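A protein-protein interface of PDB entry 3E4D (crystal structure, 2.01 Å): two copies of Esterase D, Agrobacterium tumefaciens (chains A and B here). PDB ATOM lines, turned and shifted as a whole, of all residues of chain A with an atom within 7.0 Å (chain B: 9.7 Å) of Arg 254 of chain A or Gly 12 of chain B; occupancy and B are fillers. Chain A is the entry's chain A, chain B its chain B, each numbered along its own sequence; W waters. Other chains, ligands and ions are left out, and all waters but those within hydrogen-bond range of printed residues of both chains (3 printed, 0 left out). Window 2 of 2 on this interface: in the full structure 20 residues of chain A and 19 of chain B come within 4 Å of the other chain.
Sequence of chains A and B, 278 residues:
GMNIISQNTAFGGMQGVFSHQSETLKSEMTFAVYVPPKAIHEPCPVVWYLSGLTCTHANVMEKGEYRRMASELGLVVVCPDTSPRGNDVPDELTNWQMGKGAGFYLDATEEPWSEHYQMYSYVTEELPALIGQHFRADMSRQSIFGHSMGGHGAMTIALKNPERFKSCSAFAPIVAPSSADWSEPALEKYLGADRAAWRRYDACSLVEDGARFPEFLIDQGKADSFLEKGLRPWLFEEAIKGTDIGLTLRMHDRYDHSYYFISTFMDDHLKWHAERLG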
ATOM      1  N   GLY A 221      11.325  -4.730 -23.904  1.00  0.00           N
ATOM      2  CA  GLY A 221      12.262  -5.673 -23.281  1.00  0.00           C
ATOM      3  C   GLY A 221      13.661  -5.072 -23.144  1.00  0.00           C
ATOM      4  O   GLY A 221      14.153  -4.409 -24.061  1.00  0.00           O
ATOM      5  N   LYS A 222      14.302  -5.309 -22.000  1.00  0.00           N
ATOM      6  CA  LYS A 222      15.672  -4.851 -21.764  1.00  0.00           C
ATOM      7  C   LYS A 222      16.727  -5.663 -22.531  1.00  0.00           C
ATOM      8  O   LYS A 222      17.820  -5.159 -22.821  1.00  0.00           O
ATOM      9  CB  LYS A 222      15.992  -4.853 -20.269  1.00  0.00           C
ATOM     10  CG  LYS A 222      15.213  -3.844 -19.456  1.00  0.00           C
ATOM     11  CD  LYS A 222      15.721  -3.827 -18.024  1.00  0.00           C
ATOM     12  CE  LYS A 222      14.882  -2.933 -17.132  1.00  0.00           C
ATOM     13  NZ  LYS A 222      15.176  -3.148 -15.672  1.00  0.00           N
ATOM     14  N   ALA A 223      16.411  -6.915 -22.863  1.00  0.00           N
ATOM     15  CA  ALA A 223      17.342  -7.762 -23.608  1.00  0.00           C
ATOM     16  C   ALA A 223      17.112  -7.665 -25.132  1.00  0.00           C
ATOM     17  O   ALA A 223      17.593  -8.492 -25.900  1.00  0.00           O
ATOM     18  CB  ALA A 223      17.239  -9.205 -23.128  1.00  0.00           C
ATOM     19  N   ASP A 224      16.354  -6.658 -25.555  1.00  0.00           N
ATOM     20  CA  ASP A 224      16.021  -6.446 -26.957  1.00  0.00           C
ATOM     21  C   ASP A 224      17.275  -5.950 -27.670  1.00  0.00           C
ATOM     22  O   ASP A 224      17.799  -4.894 -27.318  1.00  0.00           O
ATOM     23  CB  ASP A 224      14.901  -5.395 -27.038  1.00  0.00           C
ATOM     24  CG  ASP A 224      14.334  -5.218 -28.434  1.00  0.00           C
ATOM     25  OD1 ASP A 224      15.076  -5.360 -29.442  1.00  0.00           O
ATOM     26  OD2 ASP A 224      13.115  -4.909 -28.517  1.00  0.00           O
ATOM     27  N   HIS A 252      11.138  -4.336 -19.350  1.00  0.00           N
ATOM     28  CA  HIS A 252      11.051  -5.696 -18.818  1.00  0.00           C
ATOM     29  C   HIS A 252      12.382  -6.464 -18.869  1.00  0.00           C
ATOM     30  O   HIS A 252      12.942  -6.713 -19.944  1.00  0.00           O
ATOM     31  CB  HIS A 252       9.909  -6.461 -19.500  1.00  0.00           C
ATOM     32  CG  HIS A 252       8.589  -5.740 -19.454  1.00  0.00           C
ATOM     33  ND1 HIS A 252       7.754  -5.773 -18.352  1.00  0.00           N
ATOM     34  CD2 HIS A 252       7.972  -4.952 -20.368  1.00  0.00           C
ATOM     35  CE1 HIS A 252       6.675  -5.048 -18.597  1.00  0.00           C
ATOM     36  NE2 HIS A 252       6.782  -4.540 -19.813  1.00  0.00           N
ATOM     37  N   ASP A 253      12.898  -6.813 -17.694  1.00  0.00           N
ATOM     38  CA  ASP A 253      14.129  -7.607 -17.607  1.00  0.00           C
ATOM     39  C   ASP A 253      13.991  -8.907 -18.395  1.00  0.00           C
ATOM     40  O   ASP A 253      12.944  -9.571 -18.342  1.00  0.00           O
ATOM     41  CB  ASP A 253      14.465  -7.951 -16.152  1.00  0.00           C
ATOM     42  CG  ASP A 253      14.738  -6.726 -15.302  1.00  0.00           C
ATOM     43  OD1 ASP A 253      15.472  -5.826 -15.747  1.00  0.00           O
ATOM     44  OD2 ASP A 253      14.236  -6.680 -14.163  1.00  0.00           O
ATOM     45  N   ARG A 254      15.045  -9.247 -19.139  1.00  0.00           N
ATOM     46  CA  ARG A 254      15.162 -10.543 -19.820  1.00  0.00           C
ATOM     47  C   ARG A 254      14.318 -10.717 -21.088  1.00  0.00           C
ATOM     48  O   ARG A 254      14.591 -11.613 -21.882  1.00  0.00           O
ATOM     49  CB  ARG A 254      14.893 -11.703 -18.855  1.00  0.00           C
ATOM     50  CG  ARG A 254      15.891 -11.835 -17.704  1.00  0.00           C
ATOM     51  CD  ARG A 254      15.524 -13.029 -16.836  1.00  0.00           C
ATOM     52  NE  ARG A 254      14.120 -12.963 -16.417  1.00  0.00           N
ATOM     53  CZ  ARG A 254      13.443 -13.957 -15.838  1.00  0.00           C
ATOM     54  NH1 ARG A 254      12.166 -13.781 -15.510  1.00  0.00           N
ATOM     55  NH2 ARG A 254      14.032 -15.123 -15.583  1.00  0.00           N
ATOM     56  N   TYR A 255      13.298  -9.883 -21.276  1.00  0.00           N
ATOM     57  CA  TYR A 255      12.477  -9.971 -22.476  1.00  0.00           C
ATOM     58  C   TYR A 255      13.187  -9.342 -23.668  1.00  0.00           C
ATOM     59  O   TYR A 255      13.878  -8.350 -23.514  1.00  0.00           O
ATOM     60  CB  TYR A 255      11.107  -9.346 -22.237  1.00  0.00           C
ATOM     61  CG  TYR A 255      10.217 -10.223 -21.380  1.00  0.00           C
ATOM     62  CD1 TYR A 255       9.401 -11.195 -21.964  1.00  0.00           C
ATOM     63  CD2 TYR A 255      10.188 -10.084 -19.985  1.00  0.00           C
ATOM     64  CE1 TYR A 255       8.584 -12.008 -21.190  1.00  0.00           C
ATOM     65  CE2 TYR A 255       9.364 -10.902 -19.195  1.00  0.00           C
ATOM     66  CZ  TYR A 255       8.575 -11.859 -19.816  1.00  0.00           C
ATOM     67  OH  TYR A 255       7.759 -12.664 -19.075  1.00  0.00           O
ATOM     68  N   ASP A 256      13.009  -9.934 -24.846  1.00  0.00           N
ATOM     69  CA  ASP A 256      13.663  -9.475 -26.079  1.00  0.00           C
ATOM     70  C   ASP A 256      12.649  -8.868 -27.075  1.00  0.00           C
ATOM     71  O   ASP A 256      11.573  -8.423 -26.679  1.00  0.00           O
ATOM     72  CB  ASP A 256      14.456 -10.637 -26.705  1.00  0.00           C
ATOM     73  CG  ASP A 256      13.578 -11.859 -26.994  1.00  0.00           C
ATOM     74  OD1 ASP A 256      12.384 -11.685 -27.349  1.00  0.00           O
ATOM     75  OD2 ASP A 256      14.074 -13.000 -26.877  1.00  0.00           O
ATOM     76  N   THR A 264       3.490 -12.441 -24.313  1.00  0.00           N
ATOM     77  CA  THR A 264       3.475 -12.286 -22.865  1.00  0.00           C
ATOM     78  C   THR A 264       2.654 -11.079 -22.396  1.00  0.00           C
ATOM     79  O   THR A 264       1.844 -11.204 -21.468  1.00  0.00           O
ATOM     80  CB  THR A 264       4.890 -12.226 -22.263  1.00  0.00           C
ATOM     81  OG1 THR A 264       5.570 -13.438 -22.577  1.00  0.00           O
ATOM     82  CG2 THR A 264       4.824 -12.052 -20.725  1.00  0.00           C
ATOM     83  N   GLN B   7      16.862 -19.305 -27.451  1.00  0.00           N
ATOM     84  CA  GLN B   7      16.263 -19.160 -26.129  1.00  0.00           C
ATOM     85  C   GLN B   7      15.526 -17.829 -26.118  1.00  0.00           C
ATOM     86  O   GLN B   7      16.070 -16.812 -26.563  1.00  0.00           O
ATOM     87  CB  GLN B   7      17.327 -19.177 -25.026  1.00  0.00           C
ATOM     88  CG  GLN B   7      18.004 -20.525 -24.817  1.00  0.00           C
ATOM     89  CD  GLN B   7      19.339 -20.403 -24.105  1.00  0.00           C
ATOM     90  OE1 GLN B   7      19.967 -19.341 -24.113  1.00  0.00           O
ATOM     91  NE2 GLN B   7      19.785 -21.494 -23.490  1.00  0.00           N
ATOM     92  N   ASN B   8      14.282 -17.852 -25.650  1.00  0.00           N
ATOM     93  CA  ASN B   8      13.438 -16.658 -25.559  1.00  0.00           C
ATOM     94  C   ASN B   8      12.569 -16.701 -24.318  1.00  0.00           C
ATOM     95  O   ASN B   8      11.889 -17.691 -24.062  1.00  0.00           O
ATOM     96  CB  ASN B   8      12.526 -16.518 -26.777  1.00  0.00           C
ATOM     97  CG  ASN B   8      13.290 -16.408 -28.073  1.00  0.00           C
ATOM     98  OD1 ASN B   8      13.502 -17.403 -28.762  1.00  0.00           O
ATOM     99  ND2 ASN B   8      13.716 -15.204 -28.407  1.00  0.00           N
ATOM    100  N   THR B   9      12.590 -15.611 -23.561  1.00  0.00           N
ATOM    101  CA  THR B   9      11.760 -15.469 -22.367  1.00  0.00           C
ATOM    102  C   THR B   9      10.288 -15.267 -22.784  1.00  0.00           C
ATOM    103  O   THR B   9       9.976 -14.458 -23.656  1.00  0.00           O
ATOM    104  CB  THR B   9      12.266 -14.304 -21.475  1.00  0.00           C
ATOM    105  OG1 THR B   9      13.635 -14.547 -21.106  1.00  0.00           O
ATOM    106  CG2 THR B   9      11.429 -14.161 -20.201  1.00  0.00           C
ATOM    107  N   ALA B  10       9.400 -16.029 -22.163  1.00  0.00           N
ATOM    108  CA  ALA B  10       7.972 -15.953 -22.431  1.00  0.00           C
ATOM    109  C   ALA B  10       7.263 -16.351 -21.153  1.00  0.00           C
ATOM    110  O   ALA B  10       7.569 -17.398 -20.583  1.00  0.00           O
ATOM    111  CB  ALA B  10       7.603 -16.886 -23.569  1.00  0.00           C
ATOM    112  N   PHE B  11       6.330 -15.505 -20.708  1.00  0.00           N
ATOM    113  CA  PHE B  11       5.607 -15.663 -19.434  1.00  0.00           C
ATOM    114  C   PHE B  11       6.504 -16.057 -18.239  1.00  0.00           C
ATOM    115  O   PHE B  11       6.155 -16.940 -17.443  1.00  0.00           O
ATOM    116  CB  PHE B  11       4.452 -16.654 -19.582  1.00  0.00           C
ATOM    117  CG  PHE B  11       3.369 -16.197 -20.524  1.00  0.00           C
ATOM    118  CD1 PHE B  11       2.338 -15.370 -20.076  1.00  0.00           C
ATOM    119  CD2 PHE B  11       3.374 -16.595 -21.858  1.00  0.00           C
ATOM    120  CE1 PHE B  11       1.322 -14.951 -20.950  1.00  0.00           C
ATOM    121  CE2 PHE B  11       2.360 -16.174 -22.731  1.00  0.00           C
ATOM    122  CZ  PHE B  11       1.343 -15.354 -22.271  1.00  0.00           C
ATOM    123  N   GLY B  12       7.645 -15.388 -18.117  1.00  0.00           N
ATOM    124  CA  GLY B  12       8.572 -15.622 -17.000  1.00  0.00           C
ATOM    125  C   GLY B  12       9.391 -16.898 -17.122  1.00  0.00           C
ATOM    126  O   GLY B  12      10.302 -17.140 -16.332  1.00  0.00           O
ATOM    127  N   GLY B  13       9.059 -17.718 -18.111  1.00  0.00           N
ATOM    128  CA  GLY B  13       9.784 -18.949 -18.375  1.00  0.00           C
ATOM    129  C   GLY B  13      10.674 -18.804 -19.592  1.00  0.00           C
ATOM    130  O   GLY B  13      10.809 -17.707 -20.154  1.00  0.00           O
ATOM    131  N   MET B  14      11.279 -19.909 -20.007  1.00  0.00           N
ATOM    132  CA  MET B  14      12.194 -19.891 -21.138  1.00  0.00           C
ATOM    133  C   MET B  14      11.749 -20.889 -22.204  1.00  0.00           C
ATOM    134  O   MET B  14      11.663 -22.085 -21.945  1.00  0.00           O
ATOM    135  CB  MET B  14      13.615 -20.209 -20.648  1.00  0.00           C
ATOM    136  CG  MET B  14      14.729 -19.886 -21.640  1.00  0.00           C
ATOM    137  SD  MET B  14      15.202 -21.418 -22.762  1.00  0.00           S
ATOM    138  CE  MET B  14      16.142 -22.511 -21.441  1.00  0.00           C
ATOM    139  N   GLN B  15      11.456 -20.392 -23.398  1.00  0.00           N
ATOM    140  CA  GLN B  15      11.196 -21.268 -24.535  1.00  0.00           C
ATOM    141  C   GLN B  15      12.499 -21.456 -25.288  1.00  0.00           C
ATOM    142  O   GLN B  15      13.058 -20.492 -25.805  1.00  0.00           O
ATOM    143  CB  GLN B  15      10.159 -20.665 -25.490  1.00  0.00           C
ATOM    144  CG  GLN B  15       9.923 -21.547 -26.738  1.00  0.00           C
ATOM    145  CD  GLN B  15       9.235 -22.843 -26.394  1.00  0.00           C
ATOM    146  OE1 GLN B  15       8.104 -22.841 -25.903  1.00  0.00           O
ATOM    147  NE2 GLN B  15       9.912 -23.960 -26.628  1.00  0.00           N
ATOM    148  N   TYR B  34      10.058 -25.882 -23.248  1.00  0.00           N
ATOM    149  CA  TYR B  34       9.652 -24.704 -22.483  1.00  0.00           C
ATOM    150  C   TYR B  34       9.876 -24.996 -20.999  1.00  0.00           C
ATOM    151  O   TYR B  34       9.400 -26.004 -20.470  1.00  0.00           O
ATOM    152  CB  TYR B  34       8.174 -24.316 -22.725  1.00  0.00           C
ATOM    153  CG  TYR B  34       7.751 -23.124 -21.881  1.00  0.00           C
ATOM    154  CD1 TYR B  34       8.263 -21.847 -22.139  1.00  0.00           C
ATOM    155  CD2 TYR B  34       6.884 -23.278 -20.799  1.00  0.00           C
ATOM    156  CE1 TYR B  34       7.911 -20.757 -21.354  1.00  0.00           C
ATOM    157  CE2 TYR B  34       6.531 -22.197 -20.008  1.00  0.00           C
ATOM    158  CZ  TYR B  34       7.048 -20.939 -20.291  1.00  0.00           C
ATOM    159  OH  TYR B  34       6.689 -19.869 -19.512  1.00  0.00           O
ATOM    160  N   VAL B  35      10.619 -24.119 -20.339  1.00  0.00           N
ATOM    161  CA  VAL B  35      10.906 -24.297 -18.931  1.00  0.00           C
ATOM    162  C   VAL B  35      10.139 -23.212 -18.189  1.00  0.00           C
ATOM    163  O   VAL B  35      10.376 -22.035 -18.426  1.00  0.00           O
ATOM    164  CB  VAL B  35      12.414 -24.209 -18.632  1.00  0.00           C
ATOM    165  CG1 VAL B  35      12.674 -24.425 -17.162  1.00  0.00           C
ATOM    166  CG2 VAL B  35      13.208 -25.227 -19.467  1.00  0.00           C
ATOM    167  N   PRO B  36       9.227 -23.608 -17.283  1.00  0.00           N
ATOM    168  CA  PRO B  36       8.409 -22.638 -16.552  1.00  0.00           C
ATOM    169  C   PRO B  36       9.189 -21.964 -15.413  1.00  0.00           C
ATOM    170  O   PRO B  36      10.241 -22.475 -14.999  1.00  0.00           O
ATOM    171  CB  PRO B  36       7.274 -23.506 -15.999  1.00  0.00           C
ATOM    172  CG  PRO B  36       7.971 -24.825 -15.704  1.00  0.00           C
ATOM    173  CD  PRO B  36       8.928 -24.998 -16.871  1.00  0.00           C
ATOM    174  N   PRO B  37       8.691 -20.813 -14.914  1.00  0.00           N
ATOM    175  CA  PRO B  37       9.347 -20.130 -13.785  1.00  0.00           C
ATOM    176  C   PRO B  37       9.540 -21.001 -12.536  1.00  0.00           C
ATOM    177  O   PRO B  37      10.466 -20.761 -11.768  1.00  0.00           O
ATOM    178  CB  PRO B  37       8.424 -18.939 -13.481  1.00  0.00           C
ATOM    179  CG  PRO B  37       7.186 -19.125 -14.336  1.00  0.00           C
ATOM    180  CD  PRO B  37       7.517 -20.075 -15.427  1.00  0.00           C
ATOM    181  N   LYS B  38       8.687 -22.007 -12.345  1.00  0.00           N
ATOM    182  CA  LYS B  38       8.783 -22.907 -11.192  1.00  0.00           C
ATOM    183  C   LYS B  38      10.111 -23.674 -11.159  1.00  0.00           C
ATOM    184  O   LYS B  38      10.587 -24.042 -10.088  1.00  0.00           O
ATOM    185  CB  LYS B  38       7.612 -23.893 -11.181  1.00  0.00           C
ATOM    186  CG  LYS B  38       7.510 -24.754  -9.919  1.00  0.00           C
ATOM    187  CD  LYS B  38       6.192 -25.521  -9.841  1.00  0.00           C
ATOM    188  CE  LYS B  38       6.334 -26.943 -10.380  1.00  0.00           C
ATOM    189  NZ  LYS B  38       5.482 -27.911  -9.597  1.00  0.00           N
ATOM    190  N   ALA B  39      10.707 -23.894 -12.334  1.00  0.00           N
ATOM    191  CA  ALA B  39      11.974 -24.621 -12.456  1.00  0.00           C
ATOM    192  C   ALA B  39      13.167 -23.858 -11.909  1.00  0.00           C
ATOM    193  O   ALA B  39      14.255 -24.422 -11.783  1.00  0.00           O
ATOM    194  CB  ALA B  39      12.225 -25.004 -13.901  1.00  0.00           C
ATOM    195  N   ILE B  40      12.974 -22.576 -11.609  1.00  0.00           N
ATOM    196  CA  ILE B  40      14.006 -21.770 -10.966  1.00  0.00           C
ATOM    197  C   ILE B  40      14.283 -22.324  -9.567  1.00  0.00           C
ATOM    198  O   ILE B  40      15.427 -22.323  -9.126  1.00  0.00           O
ATOM    199  CB  ILE B  40      13.640 -20.241 -10.927  1.00  0.00           C
ATOM    200  CG1 ILE B  40      13.339 -19.738 -12.344  1.00  0.00           C
ATOM    201  CG2 ILE B  40      14.788 -19.406 -10.350  1.00  0.00           C
ATOM    202  CD1 ILE B  40      12.708 -18.350 -12.423  1.00  0.00           C
ATOM    203  N   ARG B  67       2.172 -21.749 -23.390  1.00  0.00           N
ATOM    204  CA  ARG B  67       3.134 -21.156 -22.446  1.00  0.00           C
ATOM    205  C   ARG B  67       2.518 -20.430 -21.248  1.00  0.00           C
ATOM    206  O   ARG B  67       3.075 -20.506 -20.162  1.00  0.00           O
ATOM    207  CB  ARG B  67       4.157 -20.251 -23.153  1.00  0.00           C
ATOM    208  CG  ARG B  67       5.247 -21.015 -23.917  1.00  0.00           C
ATOM    209  CD  ARG B  67       6.260 -20.072 -24.581  1.00  0.00           C
ATOM    210  NE  ARG B  67       5.666 -19.402 -25.736  1.00  0.00           N
ATOM    211  CZ  ARG B  67       5.538 -19.976 -26.929  1.00  0.00           C
ATOM    212  NH1 ARG B  67       5.977 -21.219 -27.125  1.00  0.00           N
ATOM    213  NH2 ARG B  67       4.953 -19.323 -27.918  1.00  0.00           N
ATOM    214  N   ARG B  68       1.388 -19.747 -21.452  1.00  0.00           N
ATOM    215  CA  ARG B  68       0.725 -18.988 -20.398  1.00  0.00           C
ATOM    216  C   ARG B  68       0.242 -19.914 -19.273  1.00  0.00           C
ATOM    217  O   ARG B  68       0.522 -19.664 -18.108  1.00  0.00           O
ATOM    218  CB  ARG B  68      -0.444 -18.168 -20.979  1.00  0.00           C
ATOM    219  CG  ARG B  68      -1.201 -17.277 -19.976  1.00  0.00           C
ATOM    220  CD  ARG B  68      -2.489 -16.665 -20.588  1.00  0.00           C
ATOM    221  NE  ARG B  68      -3.078 -17.545 -21.612  1.00  0.00           N
ATOM    222  CZ  ARG B  68      -3.830 -18.625 -21.363  1.00  0.00           C
ATOM    223  NH1 ARG B  68      -4.110 -18.976 -20.126  1.00  0.00           N
ATOM    224  NH2 ARG B  68      -4.294 -19.366 -22.359  1.00  0.00           N
ATOM    225  N   ALA B  70       1.161 -23.184 -19.011  1.00  0.00           N
ATOM    226  CA  ALA B  70       2.299 -24.010 -18.585  1.00  0.00           C
ATOM    227  C   ALA B  70       3.143 -23.314 -17.516  1.00  0.00           C
ATOM    228  O   ALA B  70       3.616 -23.958 -16.570  1.00  0.00           O
ATOM    229  CB  ALA B  70       3.167 -24.440 -19.779  1.00  0.00           C
ATOM    230  N   SER B  71       3.311 -21.998 -17.677  1.00  0.00           N
ATOM    231  CA  SER B  71       4.034 -21.149 -16.736  1.00  0.00           C
ATOM    232  C   SER B  71       3.272 -21.133 -15.396  1.00  0.00           C
ATOM    233  O   SER B  71       3.859 -21.377 -14.331  1.00  0.00           O
ATOM    234  CB  SER B  71       4.196 -19.732 -17.329  1.00  0.00           C
ATOM    235  OG  SER B  71       4.657 -18.787 -16.380  1.00  0.00           O
ATOM    236  N   GLU B  72       1.966 -20.898 -15.483  1.00  0.00           N
ATOM    237  CA  GLU B  72       1.078 -20.858 -14.323  1.00  0.00           C
ATOM    238  C   GLU B  72       1.054 -22.198 -13.572  1.00  0.00           C
ATOM    239  O   GLU B  72       1.125 -22.230 -12.340  1.00  0.00           O
ATOM    240  CB  GLU B  72      -0.321 -20.434 -14.769  1.00  0.00           C
ATOM    241  CG  GLU B  72      -1.415 -20.398 -13.687  1.00  0.00           C
ATOM    242  CD  GLU B  72      -2.709 -19.775 -14.217  1.00  0.00           C
ATOM    243  OE1 GLU B  72      -2.636 -18.895 -15.118  1.00  0.00           O
ATOM    244  OE2 GLU B  72      -3.798 -20.161 -13.743  1.00  0.00           O
HETATM  245  O   HOH W   1      14.438 -13.467 -23.986  1.00  0.00           O
HETATM  246  O   HOH W   2      16.750 -13.555 -26.737  1.00  0.00           O
HETATM  247  O   HOH W   3      11.312 -12.390 -24.820  1.00  0.00           O
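The backbone carbonyl oxygen (O) of Arg 254 of chain A is in hydrogen-bond range of the side-chain hydroxyl (OG1) of Thr 9 of chain B, 3.2 Å away.
OH of Tyr 255 of chain A lies within hydrogen-bond range of N of Gly 12 of chain B (2.9 Å).
The side-chain carboxylate (OD2) of Asp 256 of chain A is in hydrogen-bond range of the side-chain amide nitrogen (ND2) of Asn 8 of chain B (2.7 Å).
The side-chain hydroxyl (OG1) of Thr 264 of chain A sits at hydrogen-bond distance from the backbone NH (N) of Phe 11 of chain B, at 2.9 Å.
The backbone NH (N) of Gln 15 of chain B is in hydrogen-bond range of the backbone carbonyl oxygen (O) of Asn 8 of chain B, 2.8 Å away.
The backbone carbonyl oxygen of Ala 10 of chain B lies within hydrogen-bond range of the side-chain hydroxyl of Tyr 34 of chain B (2.8 Å).
The backbone NH of Ala 223 of chain A lies within hydrogen-bond range of the backbone carbonyl oxygen of Tyr 255 of chain A, 3.0 Å away.
O of Phe 11 of chain B sits at hydrogen-bond distance from OG of Ser 71 of chain B, at 2.6 Å.
N of Lys 222 of chain A is in hydrogen-bond range of O of Tyr 255 of chain A (3.4 Å).
NH1 of Arg 254 of chain A touches O of Gly 12 of chain B, at 3.9 Å.
CZ of Tyr 255 of chain A touches CG2 of Thr 9 of chain B, at 3.7 Å.
Tyr 255 of chain A touches Phe 11 of chain B (OH to N, 3.6 Å).
Ala 10 of chain B touches Thr 264 of chain A.
Arg 254 of chain A touches just these residues of chain B: Thr 9 (3.2 Å) and Gly 12 (3.9 Å).
Of chain B, only Thr 9 (3.7 Å), Phe 11 (3.6 Å) and Gly 12 (2.9 Å) come within 4 Å of Tyr 255 of chain A.
Of the printed residues of chain A, Phe 11 of chain B touches Tyr 255 (3.6 Å) and Thr 264 (2.9 Å).
Printed residues of chain A within 4 Å of Ala 10 of chain B: Thr 264.
Printed residues of chain A within 4 Å of Asn 8 of chain B: Asp 256 (2.7 Å).
Printed residues of chain A within 4 Å of Thr 9 of chain B: Arg 254 (3.2 Å) and Tyr 255 (3.7 Å).
Of the printed residues of chain B, Thr 264 of chain A touches Ala 10 (3.5 Å) and Phe 11 (2.9 Å).
Of the 21 printed residues of chain B, 5 touch a printed residue of chain A.
Hydrophobic or aromatic side chains of chain A within 4 Å of the printed part of chain B: Tyr 255.
Among the printed residues, 8 pairs touch across the chains.
No position is printed for both chains.
Water W3 bridges the backbone carbonyl oxygen of Thr 9 of chain B (2.7 Å) and the side-chain carboxylate of Asp 256 of chain A (2.8 Å).
Water W2 lies within hydrogen-bond range of OD2 of Asp 256 of chain A and O of Gln 7 of chain B.
Water W1 lies within hydrogen-bond range of O of Arg 254 of chain A (2.8 Å), N of Thr 9 of chain B (2.9 Å) and OD2 of Asp 256 of chain A (3.0 Å).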
